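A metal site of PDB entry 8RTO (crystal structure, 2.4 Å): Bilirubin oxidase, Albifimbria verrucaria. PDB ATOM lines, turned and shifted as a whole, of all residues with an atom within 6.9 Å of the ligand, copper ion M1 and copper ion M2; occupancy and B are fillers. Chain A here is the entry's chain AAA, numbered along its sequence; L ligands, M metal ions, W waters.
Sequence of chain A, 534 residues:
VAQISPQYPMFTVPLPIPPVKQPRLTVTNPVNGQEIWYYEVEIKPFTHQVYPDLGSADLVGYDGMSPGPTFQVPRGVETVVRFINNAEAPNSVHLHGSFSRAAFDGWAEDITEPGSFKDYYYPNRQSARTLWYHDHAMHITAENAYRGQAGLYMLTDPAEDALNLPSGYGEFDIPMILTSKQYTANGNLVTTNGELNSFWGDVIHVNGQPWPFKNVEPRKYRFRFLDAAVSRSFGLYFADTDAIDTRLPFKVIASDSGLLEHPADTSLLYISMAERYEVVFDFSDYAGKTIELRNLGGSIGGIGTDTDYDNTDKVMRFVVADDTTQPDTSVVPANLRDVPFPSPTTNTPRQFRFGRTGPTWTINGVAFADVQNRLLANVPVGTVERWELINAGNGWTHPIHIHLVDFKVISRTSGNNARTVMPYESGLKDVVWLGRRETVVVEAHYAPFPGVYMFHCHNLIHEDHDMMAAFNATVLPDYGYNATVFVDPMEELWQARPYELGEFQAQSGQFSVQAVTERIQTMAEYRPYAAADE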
ATOM      1  N   HIS A  94     -12.787  -1.705 -17.045  1.00  0.00           N
ATOM      2  CA  HIS A  94     -13.566  -0.969 -16.029  1.00  0.00           C
ATOM      3  C   HIS A  94     -15.035  -1.413 -16.065  1.00  0.00           C
ATOM      4  O   HIS A  94     -15.664  -1.262 -17.085  1.00  0.00           O
ATOM      5  CB  HIS A  94     -13.405   0.530 -16.256  1.00  0.00           C
ATOM      6  CG  HIS A  94     -14.301   1.262 -15.315  1.00  0.00           C
ATOM      7  ND1 HIS A  94     -14.317   0.983 -13.951  1.00  0.00           N
ATOM      8  CD2 HIS A  94     -15.281   2.156 -15.525  1.00  0.00           C
ATOM      9  CE1 HIS A  94     -15.228   1.741 -13.372  1.00  0.00           C
ATOM     10  NE2 HIS A  94     -15.827   2.446 -14.310  1.00  0.00           N
ATOM     11  N   LEU A  95     -15.541  -1.997 -14.961  1.00  0.00           N
ATOM     12  CA  LEU A  95     -17.000  -2.200 -14.731  1.00  0.00           C
ATOM     13  C   LEU A  95     -17.607  -0.874 -14.221  1.00  0.00           C
ATOM     14  O   LEU A  95     -17.568  -0.616 -13.000  1.00  0.00           O
ATOM     15  CB  LEU A  95     -17.281  -3.364 -13.786  1.00  0.00           C
ATOM     16  CG  LEU A  95     -18.750  -3.829 -13.725  1.00  0.00           C
ATOM     17  CD1 LEU A  95     -19.356  -4.109 -15.083  1.00  0.00           C
ATOM     18  CD2 LEU A  95     -18.924  -5.070 -12.865  1.00  0.00           C
ATOM     19  N   HIS A  96     -18.138  -0.088 -15.158  1.00  0.00           N
ATOM     20  CA  HIS A  96     -18.748   1.251 -14.938  1.00  0.00           C
ATOM     21  C   HIS A  96     -20.118   1.012 -14.284  1.00  0.00           C
ATOM     22  O   HIS A  96     -20.977   0.335 -14.907  1.00  0.00           O
ATOM     23  CB  HIS A  96     -18.767   2.043 -16.274  1.00  0.00           C
ATOM     24  CG  HIS A  96     -19.194   3.471 -16.110  1.00  0.00           C
ATOM     25  ND1 HIS A  96     -18.657   4.491 -16.872  1.00  0.00           N
ATOM     26  CD2 HIS A  96     -20.094   4.052 -15.278  1.00  0.00           C
ATOM     27  CE1 HIS A  96     -19.185   5.636 -16.497  1.00  0.00           C
ATOM     28  NE2 HIS A  96     -20.087   5.402 -15.513  1.00  0.00           N
ATOM     29  N   GLY A  97     -20.259   1.495 -13.048  1.00  0.00           N
ATOM     30  CA  GLY A  97     -21.458   1.323 -12.229  1.00  0.00           C
ATOM     31  C   GLY A  97     -21.208   0.429 -11.045  1.00  0.00           C
ATOM     32  O   GLY A  97     -22.187   0.254 -10.233  1.00  0.00           O
ATOM     33  N   ASP A 105     -11.042  -2.170 -10.622  1.00  0.00           N
ATOM     34  CA  ASP A 105     -11.932  -1.069 -11.073  1.00  0.00           C
ATOM     35  C   ASP A 105     -11.461  -0.568 -12.433  1.00  0.00           C
ATOM     36  O   ASP A 105     -12.130   0.309 -13.003  1.00  0.00           O
ATOM     37  CB  ASP A 105     -11.979   0.075 -10.072  1.00  0.00           C
ATOM     38  CG  ASP A 105     -13.045   1.102 -10.376  1.00  0.00           C
ATOM     39  OD1 ASP A 105     -14.229   0.696 -10.487  1.00  0.00           O
ATOM     40  OD2 ASP A 105     -12.681   2.292 -10.529  1.00  0.00           O
ATOM     41  N   GLY A 106     -10.353  -1.057 -12.962  1.00  0.00           N
ATOM     42  CA  GLY A 106      -9.915  -0.598 -14.301  1.00  0.00           C
ATOM     43  C   GLY A 106      -9.076   0.666 -14.253  1.00  0.00           C
ATOM     44  O   GLY A 106      -9.112   1.443 -15.252  1.00  0.00           O
ATOM     45  N   TRP A 132     -21.960  -1.179 -17.507  1.00  0.00           N
ATOM     46  CA  TRP A 132     -21.274  -1.585 -18.737  1.00  0.00           C
ATOM     47  C   TRP A 132     -19.787  -1.687 -18.462  1.00  0.00           C
ATOM     48  O   TRP A 132     -19.259  -0.950 -17.584  1.00  0.00           O
ATOM     49  CB  TRP A 132     -21.606  -0.661 -19.895  1.00  0.00           C
ATOM     50  CG  TRP A 132     -21.167   0.770 -19.743  1.00  0.00           C
ATOM     51  CD1 TRP A 132     -21.471   1.637 -18.739  1.00  0.00           C
ATOM     52  CD2 TRP A 132     -20.409   1.513 -20.698  1.00  0.00           C
ATOM     53  NE1 TRP A 132     -20.914   2.855 -18.998  1.00  0.00           N
ATOM     54  CE2 TRP A 132     -20.277   2.821 -20.213  1.00  0.00           C
ATOM     55  CE3 TRP A 132     -19.838   1.201 -21.938  1.00  0.00           C
ATOM     56  CZ2 TRP A 132     -19.590   3.814 -20.899  1.00  0.00           C
ATOM     57  CZ3 TRP A 132     -19.182   2.188 -22.630  1.00  0.00           C
ATOM     58  CH2 TRP A 132     -19.050   3.484 -22.117  1.00  0.00           C
ATOM     59  N   HIS A 134     -15.893  -1.825 -20.051  1.00  0.00           N
ATOM     60  CA  HIS A 134     -15.197  -1.229 -21.210  1.00  0.00           C
ATOM     61  C   HIS A 134     -13.741  -0.961 -20.887  1.00  0.00           C
ATOM     62  O   HIS A 134     -13.313  -0.962 -19.696  1.00  0.00           O
ATOM     63  CB  HIS A 134     -15.962   0.043 -21.649  1.00  0.00           C
ATOM     64  CG  HIS A 134     -15.926   1.165 -20.657  1.00  0.00           C
ATOM     65  ND1 HIS A 134     -14.793   1.955 -20.470  1.00  0.00           N
ATOM     66  CD2 HIS A 134     -16.886   1.697 -19.874  1.00  0.00           C
ATOM     67  CE1 HIS A 134     -15.064   2.885 -19.584  1.00  0.00           C
ATOM     68  NE2 HIS A 134     -16.361   2.761 -19.206  1.00  0.00           N
ATOM     69  N   ASP A 135     -12.968  -0.763 -21.953  1.00  0.00           N
ATOM     70  CA  ASP A 135     -11.512  -0.576 -21.836  1.00  0.00           C
ATOM     71  C   ASP A 135     -11.247   0.776 -21.195  1.00  0.00           C
ATOM     72  O   ASP A 135     -12.033   1.701 -21.502  1.00  0.00           O
ATOM     73  CB  ASP A 135     -10.796  -0.604 -23.160  1.00  0.00           C
ATOM     74  CG  ASP A 135      -9.308  -0.697 -22.866  1.00  0.00           C
ATOM     75  OD1 ASP A 135      -8.891  -1.766 -22.321  1.00  0.00           O
ATOM     76  OD2 ASP A 135      -8.617   0.323 -23.071  1.00  0.00           O
ATOM     77  N   HIS A 136     -10.205   0.859 -20.359  1.00  0.00           N
ATOM     78  CA  HIS A 136      -9.825   2.081 -19.594  1.00  0.00           C
ATOM     79  C   HIS A 136      -8.293   2.283 -19.589  1.00  0.00           C
ATOM     80  O   HIS A 136      -7.826   3.105 -18.776  1.00  0.00           O
ATOM     81  CB  HIS A 136     -10.380   2.015 -18.167  1.00  0.00           C
ATOM     82  CG  HIS A 136     -10.723   3.347 -17.607  1.00  0.00           C
ATOM     83  ND1 HIS A 136      -9.780   4.359 -17.490  1.00  0.00           N
ATOM     84  CD2 HIS A 136     -11.889   3.860 -17.182  1.00  0.00           C
ATOM     85  CE1 HIS A 136     -10.387   5.456 -17.021  1.00  0.00           C
ATOM     86  NE2 HIS A 136     -11.679   5.184 -16.842  1.00  0.00           N
ATOM     87  N   THR A 141      -7.693   4.333 -24.475  1.00  0.00           N
ATOM     88  CA  THR A 141      -9.148   4.154 -24.190  1.00  0.00           C
ATOM     89  C   THR A 141     -10.018   4.501 -25.429  1.00  0.00           C
ATOM     90  O   THR A 141     -10.792   3.626 -25.884  1.00  0.00           O
ATOM     91  CB  THR A 141      -9.499   4.971 -22.930  1.00  0.00           C
ATOM     92  OG1 THR A 141      -8.719   4.475 -21.836  1.00  0.00           O
ATOM     93  CG2 THR A 141     -10.966   4.936 -22.565  1.00  0.00           C
ATOM     94  N   ALA A 274     -21.515   7.715 -21.684  1.00  0.00           N
ATOM     95  CA  ALA A 274     -21.433   6.767 -20.549  1.00  0.00           C
ATOM     96  C   ALA A 274     -22.666   6.880 -19.656  1.00  0.00           C
ATOM     97  O   ALA A 274     -22.784   6.076 -18.654  1.00  0.00           O
ATOM     98  CB  ALA A 274     -20.152   7.002 -19.801  1.00  0.00           C
ATOM     99  N   ARG A 276     -26.399   6.017 -18.757  1.00  0.00           N
ATOM    100  CA  ARG A 276     -27.450   4.956 -18.897  1.00  0.00           C
ATOM    101  C   ARG A 276     -28.804   5.518 -18.445  1.00  0.00           C
ATOM    102  O   ARG A 276     -28.912   5.926 -17.233  1.00  0.00           O
ATOM    103  CB  ARG A 276     -27.117   3.709 -18.047  1.00  0.00           C
ATOM    104  CG  ARG A 276     -25.981   2.870 -18.600  1.00  0.00           C
ATOM    105  CD  ARG A 276     -24.610   3.345 -18.130  1.00  0.00           C
ATOM    106  NE  ARG A 276     -24.447   3.070 -16.707  1.00  0.00           N
ATOM    107  CZ  ARG A 276     -23.778   3.838 -15.833  1.00  0.00           C
ATOM    108  NH1 ARG A 276     -23.783   3.469 -14.562  1.00  0.00           N
ATOM    109  NH2 ARG A 276     -23.117   4.947 -16.195  1.00  0.00           N
ATOM    110  N   HIS A 401     -17.485  11.673 -15.125  1.00  0.00           N
ATOM    111  CA  HIS A 401     -17.579  10.394 -14.398  1.00  0.00           C
ATOM    112  C   HIS A 401     -16.709  10.411 -13.133  1.00  0.00           C
ATOM    113  O   HIS A 401     -15.507  10.635 -13.262  1.00  0.00           O
ATOM    114  CB  HIS A 401     -17.164   9.269 -15.353  1.00  0.00           C
ATOM    115  CG  HIS A 401     -17.322   7.937 -14.739  1.00  0.00           C
ATOM    116  ND1 HIS A 401     -18.327   7.682 -13.803  1.00  0.00           N
ATOM    117  CD2 HIS A 401     -16.599   6.816 -14.878  1.00  0.00           C
ATOM    118  CE1 HIS A 401     -18.219   6.426 -13.411  1.00  0.00           C
ATOM    119  NE2 HIS A 401     -17.165   5.868 -14.080  1.00  0.00           N
ATOM    120  N   ILE A 402     -17.292  10.093 -11.976  1.00  0.00           N
ATOM    121  CA  ILE A 402     -16.564   9.756 -10.718  1.00  0.00           C
ATOM    122  C   ILE A 402     -16.693   8.246 -10.468  1.00  0.00           C
ATOM    123  O   ILE A 402     -17.837   7.739 -10.318  1.00  0.00           O
ATOM    124  CB  ILE A 402     -17.116  10.586  -9.534  1.00  0.00           C
ATOM    125  CG1 ILE A 402     -17.259  12.062  -9.953  1.00  0.00           C
ATOM    126  CG2 ILE A 402     -16.262  10.457  -8.291  1.00  0.00           C
ATOM    127  CD1 ILE A 402     -17.932  12.933  -8.963  1.00  0.00           C
ATOM    128  N   HIS A 403     -15.571   7.519 -10.399  1.00  0.00           N
ATOM    129  CA  HIS A 403     -15.544   6.085 -10.031  1.00  0.00           C
ATOM    130  C   HIS A 403     -15.997   5.955  -8.562  1.00  0.00           C
ATOM    131  O   HIS A 403     -16.031   7.016  -7.844  1.00  0.00           O
ATOM    132  CB  HIS A 403     -14.142   5.547 -10.302  1.00  0.00           C
ATOM    133  CG  HIS A 403     -13.794   5.365 -11.744  1.00  0.00           C
ATOM    134  ND1 HIS A 403     -13.373   4.150 -12.253  1.00  0.00           N
ATOM    135  CD2 HIS A 403     -13.832   6.228 -12.791  1.00  0.00           C
ATOM    136  CE1 HIS A 403     -13.135   4.266 -13.554  1.00  0.00           C
ATOM    137  NE2 HIS A 403     -13.410   5.545 -13.919  1.00  0.00           N
ATOM    138  N   VAL A 431     -22.344   9.582 -13.924  1.00  0.00           N
ATOM    139  CA  VAL A 431     -21.952  10.558 -14.972  1.00  0.00           C
ATOM    140  C   VAL A 431     -22.914  11.753 -14.921  1.00  0.00           C
ATOM    141  O   VAL A 431     -24.156  11.499 -14.819  1.00  0.00           O
ATOM    142  CB  VAL A 431     -21.951   9.929 -16.372  1.00  0.00           C
ATOM    143  CG1 VAL A 431     -21.461  10.903 -17.427  1.00  0.00           C
ATOM    144  CG2 VAL A 431     -21.132   8.638 -16.433  1.00  0.00           C
ATOM    145  N   MET A 454     -10.398   6.788  -9.997  1.00  0.00           N
ATOM    146  CA  MET A 454     -10.309   7.777 -11.089  1.00  0.00           C
ATOM    147  C   MET A 454     -11.572   8.637 -11.127  1.00  0.00           C
ATOM    148  O   MET A 454     -12.656   8.228 -10.686  1.00  0.00           O
ATOM    149  CB  MET A 454     -10.133   7.100 -12.440  1.00  0.00           C
ATOM    150  CG  MET A 454      -8.706   6.618 -12.660  1.00  0.00           C
ATOM    151  SD  MET A 454      -8.447   5.758 -14.212  1.00  0.00           S
ATOM    152  CE  MET A 454      -9.814   4.591 -14.113  1.00  0.00           C
ATOM    153  N   PHE A 455     -11.414   9.826 -11.655  1.00  0.00           N
ATOM    154  CA  PHE A 455     -12.538  10.619 -12.147  1.00  0.00           C
ATOM    155  C   PHE A 455     -12.029  11.396 -13.336  1.00  0.00           C
ATOM    156  O   PHE A 455     -10.801  11.725 -13.382  1.00  0.00           O
ATOM    157  CB  PHE A 455     -13.151  11.491 -11.052  1.00  0.00           C
ATOM    158  CG  PHE A 455     -12.420  12.750 -10.708  1.00  0.00           C
ATOM    159  CD1 PHE A 455     -11.392  12.736  -9.773  1.00  0.00           C
ATOM    160  CD2 PHE A 455     -12.842  13.974 -11.212  1.00  0.00           C
ATOM    161  CE1 PHE A 455     -10.777  13.905  -9.368  1.00  0.00           C
ATOM    162  CE2 PHE A 455     -12.227  15.139 -10.816  1.00  0.00           C
ATOM    163  CZ  PHE A 455     -11.175  15.103  -9.906  1.00  0.00           C
ATOM    164  N   HIS A 456     -12.959  11.694 -14.241  1.00  0.00           N
ATOM    165  CA  HIS A 456     -12.581  12.238 -15.557  1.00  0.00           C
ATOM    166  C   HIS A 456     -13.797  12.575 -16.399  1.00  0.00           C
ATOM    167  O   HIS A 456     -14.926  12.190 -16.052  1.00  0.00           O
ATOM    168  CB  HIS A 456     -11.787  11.161 -16.292  1.00  0.00           C
ATOM    169  CG  HIS A 456     -12.539   9.899 -16.469  1.00  0.00           C
ATOM    170  ND1 HIS A 456     -13.130   9.552 -17.656  1.00  0.00           N
ATOM    171  CD2 HIS A 456     -12.740   8.865 -15.621  1.00  0.00           C
ATOM    172  CE1 HIS A 456     -13.688   8.367 -17.522  1.00  0.00           C
ATOM    173  NE2 HIS A 456     -13.423   7.922 -16.296  1.00  0.00           N
ATOM    174  N   CYS A 457     -13.508  13.183 -17.538  1.00  0.00           N
ATOM    175  CA  CYS A 457     -14.448  13.375 -18.636  1.00  0.00           C
ATOM    176  C   CYS A 457     -14.552  12.057 -19.416  1.00  0.00           C
ATOM    177  O   CYS A 457     -13.500  11.404 -19.549  1.00  0.00           O
ATOM    178  CB  CYS A 457     -13.926  14.514 -19.493  1.00  0.00           C
ATOM    179  SG  CYS A 457     -14.984  14.789 -20.924  1.00  0.00           S
ATOM    180  N   HIS A 458     -15.747  11.697 -19.930  1.00  0.00           N
ATOM    181  CA  HIS A 458     -16.011  10.431 -20.652  1.00  0.00           C
ATOM    182  C   HIS A 458     -16.195  10.674 -22.158  1.00  0.00           C
ATOM    183  O   HIS A 458     -16.510   9.678 -22.852  1.00  0.00           O
ATOM    184  CB  HIS A 458     -17.250   9.697 -20.097  1.00  0.00           C
ATOM    185  CG  HIS A 458     -17.090   8.217 -20.006  1.00  0.00           C
ATOM    186  ND1 HIS A 458     -17.012   7.411 -21.115  1.00  0.00           N
ATOM    187  CD2 HIS A 458     -16.944   7.404 -18.936  1.00  0.00           C
ATOM    188  CE1 HIS A 458     -16.870   6.144 -20.733  1.00  0.00           C
ATOM    189  NE2 HIS A 458     -16.834   6.116 -19.396  1.00  0.00           N
ATOM    190  N   LEU A 460     -13.975  10.382 -24.792  1.00  0.00           N
ATOM    191  CA  LEU A 460     -12.795   9.507 -24.631  1.00  0.00           C
ATOM    192  C   LEU A 460     -11.580  10.206 -25.245  1.00  0.00           C
ATOM    193  O   LEU A 460     -10.484   9.963 -24.730  1.00  0.00           O
ATOM    194  CB  LEU A 460     -13.092   8.149 -25.277  1.00  0.00           C
ATOM    195  CG  LEU A 460     -14.303   7.441 -24.659  1.00  0.00           C
ATOM    196  CD1 LEU A 460     -14.493   6.068 -25.297  1.00  0.00           C
ATOM    197  CD2 LEU A 460     -14.146   7.331 -23.144  1.00  0.00           C
ATOM    198  N   GLU A 463     -10.465  12.439 -22.305  1.00  0.00           N
ATOM    199  CA  GLU A 463      -9.949  11.494 -21.275  1.00  0.00           C
ATOM    200  C   GLU A 463      -8.507  11.142 -21.631  1.00  0.00           C
ATOM    201  O   GLU A 463      -7.684  11.122 -20.730  1.00  0.00           O
ATOM    202  CB  GLU A 463     -10.827  10.245 -21.237  1.00  0.00           C
ATOM    203  CG  GLU A 463     -10.480   9.250 -20.127  1.00  0.00           C
ATOM    204  CD  GLU A 463     -11.426   8.054 -20.019  1.00  0.00           C
ATOM    205  OE1 GLU A 463     -12.666   8.262 -20.122  1.00  0.00           O
ATOM    206  OE2 GLU A 463     -10.926   6.919 -19.803  1.00  0.00           O
ATOM    207  N   MET A 468      -8.210  13.524 -16.940  1.00  0.00           N
ATOM    208  CA  MET A 468      -8.466  12.505 -15.897  1.00  0.00           C
ATOM    209  C   MET A 468      -7.640  12.881 -14.656  1.00  0.00           C
ATOM    210  O   MET A 468      -6.625  13.589 -14.795  1.00  0.00           O
ATOM    211  CB  MET A 468      -8.094  11.142 -16.479  1.00  0.00           C
ATOM    212  CG  MET A 468      -8.522   9.963 -15.657  1.00  0.00           C
ATOM    213  SD  MET A 468      -8.776   8.472 -16.720  1.00  0.00           S
ATOM    214  CE  MET A 468      -7.048   8.112 -17.087  1.00  0.00           C
HETATM  215  O1  LIG L   1     -15.251   5.130 -16.808  1.00  0.00           O
HETATM  216  O2  LIG L   1     -14.493   5.103 -17.708  1.00  0.00           O
HETATM  217 CU    CU M   1     -17.138   4.253 -18.338  1.00  0.00          CU
HETATM  218 CU    CU M   2     -13.304   5.908 -15.833  1.00  0.00          CU
HETATM  219 CU    CU M   3     -16.564   4.251 -14.275  1.00  0.00          CU
HETATM  220  O   HOH W   1     -13.845   5.160 -20.752  1.00  0.00           O
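O of Met 454 is in hydrogen-bond range of N of His 403 (3.0 Å). A ring nitrogen (ND1) of His 456 lies close to the side-chain carboxylate (OE1) of Glu 463 (2.8 Å). O of His 136 sits close to OG1 of Thr 141, 3.5 Å away. A ring nitrogen (ND1) of His 94 sits at hydrogen-bond distance from the backbone carbonyl oxygen (O) of Asp 105. N of His 401 is in hydrogen-bond range of O of His 456 (2.8 Å). N of His 96 lies within hydrogen-bond range of O of Trp 132. ND1 of His 401 lies close to NE2 of His 96 (3.3 Å). O of His 134 lies within hydrogen-bond range of N of His 94 (2.8 Å).
An oxygen (O1) of the ligand sits close to a ring nitrogen (NE2) of His 401. Merely in contact with the ligand: His 94. Hydrophobic or aromatic side chains that line the ligand: His 94, His 96, His 134, His 136, His 401, His 403, His 456 and His 458.
Residues that only touch copper ion M1: Trp 132 and His 94. Along chain A the residues within 4 Å of copper ion M1 span positions 94 to 458.
Residues that only touch copper ion M2: His 401 (3.5 Å). Of the 25 residues printed, 4 come within 4 Å of copper ion M2. The nearest printed residue that does not touch copper ion M2 is Met 454 (4.1 Å).
Copper ion M1 is bound by a ring nitrogen (NE2) of His 134 (1.9 Å), a ring nitrogen (ND1) of His 96 (2.1 Å), a ring nitrogen (NE2) of His 458 (2.2 Å) and an oxygen (O1) of the ligand (2.6 Å). Copper ion M1 has four donor atoms within binding distance.
Copper ion M2 is bound by a ring nitrogen (NE2) of His 403, a ring nitrogen (NE2) of His 136, a ring nitrogen (NE2) of His 456 and an oxygen (O1) of the ligand. Copper ion M2 has four donor atoms within binding distance.
Water W1 lies within hydrogen-bond range of a ring nitrogen (ND1) of His 134 (3.4 Å) and the side-chain carboxylate (OE1) of Glu 463 (3.4 Å).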
